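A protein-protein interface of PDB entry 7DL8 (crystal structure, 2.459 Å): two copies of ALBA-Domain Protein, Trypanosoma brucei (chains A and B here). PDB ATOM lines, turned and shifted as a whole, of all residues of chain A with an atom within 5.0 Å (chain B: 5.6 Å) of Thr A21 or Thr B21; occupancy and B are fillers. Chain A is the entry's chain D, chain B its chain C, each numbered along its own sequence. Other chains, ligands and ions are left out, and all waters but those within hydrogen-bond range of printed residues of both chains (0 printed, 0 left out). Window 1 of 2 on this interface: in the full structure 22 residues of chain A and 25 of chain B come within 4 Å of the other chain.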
ATOM      1  N   VAL A  16      20.661 -14.435   8.948  1.00  0.00           N
ATOM      2  CA  VAL A  16      20.054 -15.296   9.953  1.00  0.00           C
ATOM      3  C   VAL A  16      21.154 -15.948  10.776  1.00  0.00           C
ATOM      4  O   VAL A  16      22.094 -16.533  10.225  1.00  0.00           O
ATOM      5  CB  VAL A  16      19.158 -16.356   9.289  1.00  0.00           C
ATOM      6  CG1 VAL A  16      18.545 -17.274  10.337  1.00  0.00           C
ATOM      7  CG2 VAL A  16      18.076 -15.690   8.453  1.00  0.00           C
ATOM      8  N   GLY A  17      21.045 -15.845  12.097  1.00  0.00           N
ATOM      9  CA  GLY A  17      22.064 -16.409  12.959  1.00  0.00           C
ATOM     10  C   GLY A  17      21.530 -16.600  14.361  1.00  0.00           C
ATOM     11  O   GLY A  17      20.371 -16.300  14.659  1.00  0.00           O
ATOM     12  N   TYR A  18      22.404 -17.106  15.225  1.00  0.00           N
ATOM     13  CA  TYR A  18      22.024 -17.496  16.575  1.00  0.00           C
ATOM     14  C   TYR A  18      22.344 -16.459  17.644  1.00  0.00           C
ATOM     15  O   TYR A  18      21.880 -16.610  18.780  1.00  0.00           O
ATOM     16  CB  TYR A  18      22.671 -18.839  16.918  1.00  0.00           C
ATOM     17  CG  TYR A  18      22.361 -19.885  15.872  1.00  0.00           C
ATOM     18  CD1 TYR A  18      21.078 -20.008  15.350  1.00  0.00           C
ATOM     19  CD2 TYR A  18      23.348 -20.730  15.387  1.00  0.00           C
ATOM     20  CE1 TYR A  18      20.787 -20.949  14.385  1.00  0.00           C
ATOM     21  CE2 TYR A  18      23.064 -21.680  14.426  1.00  0.00           C
ATOM     22  CZ  TYR A  18      21.783 -21.786  13.930  1.00  0.00           C
ATOM     23  OH  TYR A  18      21.502 -22.731  12.972  1.00  0.00           O
ATOM     24  N   ARG A  19      23.127 -15.427  17.332  1.00  0.00           N
ATOM     25  CA  ARG A  19      23.424 -14.410  18.333  1.00  0.00           C
ATOM     26  C   ARG A  19      22.149 -13.638  18.643  1.00  0.00           C
ATOM     27  O   ARG A  19      21.526 -13.060  17.746  1.00  0.00           O
ATOM     28  CB  ARG A  19      24.526 -13.469  17.853  1.00  0.00           C
ATOM     29  CG  ARG A  19      25.087 -12.599  18.973  1.00  0.00           C
ATOM     30  CD  ARG A  19      25.860 -11.404  18.446  1.00  0.00           C
ATOM     31  NE  ARG A  19      26.705 -10.812  19.479  1.00  0.00           N
ATOM     32  CZ  ARG A  19      26.455  -9.651  20.076  1.00  0.00           C
ATOM     33  NH1 ARG A  19      25.380  -8.950  19.742  1.00  0.00           N
ATOM     34  NH2 ARG A  19      27.278  -9.190  21.007  1.00  0.00           N
ATOM     35  N   GLY A  20      21.762 -13.634  19.912  1.00  0.00           N
ATOM     36  CA  GLY A  20      20.517 -13.020  20.327  1.00  0.00           C
ATOM     37  C   GLY A  20      19.620 -14.121  20.845  1.00  0.00           C
ATOM     38  O   GLY A  20      18.948 -13.970  21.870  1.00  0.00           O
ATOM     39  N   THR A  21      19.634 -15.257  20.144  1.00  0.00           N
ATOM     40  CA  THR A  21      18.897 -16.421  20.617  1.00  0.00           C
ATOM     41  C   THR A  21      19.609 -17.037  21.812  1.00  0.00           C
ATOM     42  O   THR A  21      18.966 -17.470  22.775  1.00  0.00           O
ATOM     43  CB  THR A  21      18.745 -17.446  19.490  1.00  0.00           C
ATOM     44  OG1 THR A  21      18.071 -16.843  18.378  1.00  0.00           O
ATOM     45  CG2 THR A  21      17.953 -18.657  19.965  1.00  0.00           C
ATOM     46  N   LYS A  22      20.943 -17.070  21.767  1.00  0.00           N
ATOM     47  CA  LYS A  22      21.710 -17.520  22.923  1.00  0.00           C
ATOM     48  C   LYS A  22      21.532 -16.561  24.092  1.00  0.00           C
ATOM     49  O   LYS A  22      21.502 -16.985  25.254  1.00  0.00           O
ATOM     50  CB  LYS A  22      23.189 -17.644  22.557  1.00  0.00           C
ATOM     51  CG  LYS A  22      23.483 -18.602  21.415  1.00  0.00           C
ATOM     52  CD  LYS A  22      24.969 -18.613  21.078  1.00  0.00           C
ATOM     53  CE  LYS A  22      25.231 -18.038  19.694  1.00  0.00           C
ATOM     54  NZ  LYS A  22      26.529 -17.309  19.624  1.00  0.00           N
ATOM     55  N   PHE A  23      21.407 -15.263  23.802  1.00  0.00           N
ATOM     56  CA  PHE A  23      21.210 -14.276  24.859  1.00  0.00           C
ATOM     57  C   PHE A  23      19.851 -14.441  25.528  1.00  0.00           C
ATOM     58  O   PHE A  23      19.727 -14.248  26.744  1.00  0.00           O
ATOM     59  CB  PHE A  23      21.360 -12.865  24.293  1.00  0.00           C
ATOM     60  CG  PHE A  23      22.786 -12.417  24.155  1.00  0.00           C
ATOM     61  CD1 PHE A  23      23.536 -12.094  25.274  1.00  0.00           C
ATOM     62  CD2 PHE A  23      23.378 -12.321  22.906  1.00  0.00           C
ATOM     63  CE1 PHE A  23      24.849 -11.681  25.150  1.00  0.00           C
ATOM     64  CE2 PHE A  23      24.691 -11.910  22.776  1.00  0.00           C
ATOM     65  CZ  PHE A  23      25.428 -11.590  23.899  1.00  0.00           C
ATOM     66  N   LEU A  24      18.822 -14.788  24.753  1.00  0.00           N
ATOM     67  CA  LEU A  24      17.494 -14.983  25.327  1.00  0.00           C
ATOM     68  C   LEU A  24      17.494 -16.132  26.326  1.00  0.00           C
ATOM     69  O   LEU A  24      16.951 -16.013  27.429  1.00  0.00           O
ATOM     70  CB  LEU A  24      16.473 -15.231  24.217  1.00  0.00           C
ATOM     71  N   PHE A  25      18.113 -17.255  25.957  1.00  0.00           N
ATOM     72  CA  PHE A  25      18.154 -18.403  26.856  1.00  0.00           C
ATOM     73  C   PHE A  25      19.122 -18.178  28.010  1.00  0.00           C
ATOM     74  O   PHE A  25      18.929 -18.739  29.095  1.00  0.00           O
ATOM     75  CB  PHE A  25      18.505 -19.665  26.071  1.00  0.00           C
ATOM     76  CG  PHE A  25      17.445 -20.069  25.088  1.00  0.00           C
ATOM     77  CD1 PHE A  25      16.164 -20.369  25.520  1.00  0.00           C
ATOM     78  CD2 PHE A  25      17.721 -20.133  23.733  1.00  0.00           C
ATOM     79  CE1 PHE A  25      15.180 -20.735  24.622  1.00  0.00           C
ATOM     80  CE2 PHE A  25      16.741 -20.497  22.828  1.00  0.00           C
ATOM     81  CZ  PHE A  25      15.469 -20.800  23.274  1.00  0.00           C
ATOM     82  N   VAL B  16      16.625 -24.949  24.426  1.00  0.00           N
ATOM     83  CA  VAL B  16      17.247 -24.038  23.475  1.00  0.00           C
ATOM     84  C   VAL B  16      16.880 -24.477  22.065  1.00  0.00           C
ATOM     85  O   VAL B  16      17.057 -25.646  21.701  1.00  0.00           O
ATOM     86  CB  VAL B  16      18.772 -24.010  23.670  1.00  0.00           C
ATOM     87  CG1 VAL B  16      19.431 -23.139  22.611  1.00  0.00           C
ATOM     88  CG2 VAL B  16      19.123 -23.522  25.067  1.00  0.00           C
ATOM     89  N   GLY B  17      16.366 -23.545  21.267  1.00  0.00           N
ATOM     90  CA  GLY B  17      15.956 -23.901  19.924  1.00  0.00           C
ATOM     91  C   GLY B  17      15.825 -22.691  19.027  1.00  0.00           C
ATOM     92  O   GLY B  17      16.053 -21.549  19.434  1.00  0.00           O
ATOM     93  N   TYR B  18      15.438 -22.972  17.786  1.00  0.00           N
ATOM     94  CA  TYR B  18      15.381 -22.007  16.696  1.00  0.00           C
ATOM     95  C   TYR B  18      13.994 -21.432  16.430  1.00  0.00           C
ATOM     96  O   TYR B  18      13.870 -20.549  15.575  1.00  0.00           O
ATOM     97  CB  TYR B  18      15.937 -22.635  15.418  1.00  0.00           C
ATOM     98  CG  TYR B  18      17.322 -23.205  15.596  1.00  0.00           C
ATOM     99  CD1 TYR B  18      18.263 -22.562  16.391  1.00  0.00           C
ATOM    100  CD2 TYR B  18      17.689 -24.388  14.975  1.00  0.00           C
ATOM    101  CE1 TYR B  18      19.530 -23.083  16.561  1.00  0.00           C
ATOM    102  CE2 TYR B  18      18.955 -24.914  15.134  1.00  0.00           C
ATOM    103  CZ  TYR B  18      19.871 -24.257  15.927  1.00  0.00           C
ATOM    104  OH  TYR B  18      21.132 -24.784  16.084  1.00  0.00           O
ATOM    105  N   ARG B  19      12.953 -21.910  17.118  1.00  0.00           N
ATOM    106  CA  ARG B  19      11.597 -21.474  16.790  1.00  0.00           C
ATOM    107  C   ARG B  19      11.436 -19.967  16.947  1.00  0.00           C
ATOM    108  O   ARG B  19      10.844 -19.309  16.084  1.00  0.00           O
ATOM    109  CB  ARG B  19      10.583 -22.211  17.665  1.00  0.00           C
ATOM    110  N   GLY B  20      11.967 -19.396  18.030  1.00  0.00           N
ATOM    111  CA  GLY B  20      11.865 -17.959  18.204  1.00  0.00           C
ATOM    112  C   GLY B  20      12.810 -17.178  17.316  1.00  0.00           C
ATOM    113  O   GLY B  20      12.643 -15.964  17.165  1.00  0.00           O
ATOM    114  N   THR B  21      13.739 -17.867  16.651  1.00  0.00           N
ATOM    115  CA  THR B  21      14.692 -17.196  15.777  1.00  0.00           C
ATOM    116  C   THR B  21      14.145 -17.083  14.365  1.00  0.00           C
ATOM    117  O   THR B  21      14.318 -16.050  13.708  1.00  0.00           O
ATOM    118  CB  THR B  21      16.019 -17.966  15.760  1.00  0.00           C
ATOM    119  OG1 THR B  21      16.561 -18.042  17.085  1.00  0.00           O
ATOM    120  CG2 THR B  21      17.031 -17.301  14.831  1.00  0.00           C
ATOM    121  N   LYS B  22      13.480 -18.132  13.886  1.00  0.00           N
ATOM    122  CA  LYS B  22      12.859 -18.068  12.570  1.00  0.00           C
ATOM    123  C   LYS B  22      11.710 -17.066  12.543  1.00  0.00           C
ATOM    124  O   LYS B  22      11.523 -16.359  11.546  1.00  0.00           O
ATOM    125  CB  LYS B  22      12.373 -19.457  12.166  1.00  0.00           C
ATOM    126  CG  LYS B  22      13.471 -20.507  12.146  1.00  0.00           C
ATOM    127  CD  LYS B  22      12.918 -21.869  11.762  1.00  0.00           C
ATOM    128  CE  LYS B  22      12.979 -22.851  12.919  1.00  0.00           C
ATOM    129  NZ  LYS B  22      11.884 -23.860  12.842  1.00  0.00           N
ATOM    130  N   PHE B  23      10.940 -16.975  13.632  1.00  0.00           N
ATOM    131  CA  PHE B  23       9.831 -16.024  13.665  1.00  0.00           C
ATOM    132  C   PHE B  23      10.333 -14.586  13.681  1.00  0.00           C
ATOM    133  O   PHE B  23       9.707 -13.698  13.090  1.00  0.00           O
ATOM    134  CB  PHE B  23       8.931 -16.298  14.870  1.00  0.00           C
ATOM    135  CG  PHE B  23       7.882 -17.344  14.614  1.00  0.00           C
ATOM    136  CD1 PHE B  23       6.863 -17.116  13.705  1.00  0.00           C
ATOM    137  CD2 PHE B  23       7.917 -18.556  15.283  1.00  0.00           C
ATOM    138  CE1 PHE B  23       5.898 -18.077  13.467  1.00  0.00           C
ATOM    139  CE2 PHE B  23       6.955 -19.522  15.049  1.00  0.00           C
ATOM    140  CZ  PHE B  23       5.944 -19.282  14.139  1.00  0.00           C
ATOM    141  N   LEU B  24      11.460 -14.339  14.348  1.00  0.00           N
ATOM    142  CA  LEU B  24      12.021 -12.992  14.384  1.00  0.00           C
ATOM    143  C   LEU B  24      12.523 -12.569  13.010  1.00  0.00           C
ATOM    144  O   LEU B  24      12.258 -11.451  12.556  1.00  0.00           O
ATOM    145  CB  LEU B  24      13.149 -12.924  15.414  1.00  0.00           C
ATOM    146  CG  LEU B  24      14.099 -11.734  15.275  1.00  0.00           C
ATOM    147  CD1 LEU B  24      13.389 -10.444  15.655  1.00  0.00           C
ATOM    148  CD2 LEU B  24      15.350 -11.938  16.117  1.00  0.00           C
ATOM    149  N   PHE B  25      13.252 -13.456  12.328  1.00  0.00           N
ATOM    150  CA  PHE B  25      13.814 -13.103  11.029  1.00  0.00           C
ATOM    151  C   PHE B  25      12.743 -13.044   9.948  1.00  0.00           C
ATOM    152  O   PHE B  25      12.887 -12.292   8.977  1.00  0.00           O
ATOM    153  CB  PHE B  25      14.926 -14.082  10.660  1.00  0.00           C
ATOM    154  CG  PHE B  25      16.215 -13.817  11.384  1.00  0.00           C
ATOM    155  CD1 PHE B  25      16.889 -12.621  11.202  1.00  0.00           C
ATOM    156  CD2 PHE B  25      16.740 -14.749  12.263  1.00  0.00           C
ATOM    157  CE1 PHE B  25      18.070 -12.364  11.871  1.00  0.00           C
ATOM    158  CE2 PHE B  25      17.922 -14.496  12.936  1.00  0.00           C
ATOM    159  CZ  PHE B  25      18.587 -13.302  12.738  1.00  0.00           C
ATOM    160  N   VAL B  26      11.673 -13.830  10.086  1.00  0.00           N
ATOM    161  CA  VAL B  26      10.520 -13.665   9.206  1.00  0.00           C
ATOM    162  C   VAL B  26       9.899 -12.291   9.422  1.00  0.00           C
ATOM    163  O   VAL B  26       9.520 -11.601   8.467  1.00  0.00           O
ATOM    164  CB  VAL B  26       9.501 -14.797   9.435  1.00  0.00           C
ATOM    165  CG1 VAL B  26       8.127 -14.403   8.912  1.00  0.00           C
ATOM    166  CG2 VAL B  26       9.975 -16.080   8.769  1.00  0.00           C
ATOM    167  N   VAL B  55      13.056 -19.930   7.074  1.00  0.00           N
ATOM    168  CA  VAL B  55      12.555 -18.563   7.203  1.00  0.00           C
ATOM    169  C   VAL B  55      11.937 -18.105   5.889  1.00  0.00           C
ATOM    170  O   VAL B  55      10.907 -17.418   5.870  1.00  0.00           O
ATOM    171  CB  VAL B  55      13.690 -17.623   7.657  1.00  0.00           C
ATOM    172  CG1 VAL B  55      13.442 -16.190   7.194  1.00  0.00           C
ATOM    173  CG2 VAL B  55      13.860 -17.676   9.166  1.00  0.00           C
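OG1 of Thr B21 lies close to OG1 of Thr A21, 2.3 Å away.
Val A16 touches Phe B25. O of Gly A17 touches CG2 of Thr B21, 3.5 Å away. Gly A17 touches Phe B25 (O to CE2, 3.5 Å). Tyr B18 touches Tyr A18. Gly B17 touches Thr A21. CE2 of Phe A25 touches CA of Val B16, 3.6 Å away. Gly B17 touches Phe A25.
Thr A21 touches just these residues of chain B: Gly B17 (3.5 Å) and Thr B21 (2.3 Å). Of the printed residues of chain B, Gly A17 touches Thr B21 and Phe B25. Of the printed residues of chain A, Phe B25 touches Val A16 (3.7 Å) and Gly A17 (3.5 Å). Of the printed residues of chain B, Phe A25 touches Val B16 (3.6 Å) and Gly B17 (3.4 Å). Printed residues of chain A within 4 Å of Gly B17: Thr A21 and Phe A25. Of the printed residues of chain A, Tyr B18 touches Tyr A18. Val B26 touches none of the printed residues of chain A.
Val A16 touches Phe B25, and with the chains exchanged Phe A25 touches Val B16. Gly A17 touches Phe B25, and with the chains exchanged Phe A25 touches Gly B17. Tyr A18 touches its own counterpart, Tyr B18. Thr A21 touches its own counterpart, Thr B21. Of the 8 pairs that touch across the chains among the printed residues, 8 have their exchanged pair printed and touching as well.
Of the 12 printed residues of chain B, 5 touch a printed residue of chain A. Hydrophobic or aromatic side chains of chain B within 4 Å of the printed part of chain A: Val B16, Tyr B18 and Phe B25. Of the 10 printed residues of chain A, 5 touch a printed residue of chain B. Among the printed residues, no Asp or Glu carboxylate lies within 4 Å of a Lys or Arg side-chain nitrogen of the other chain.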
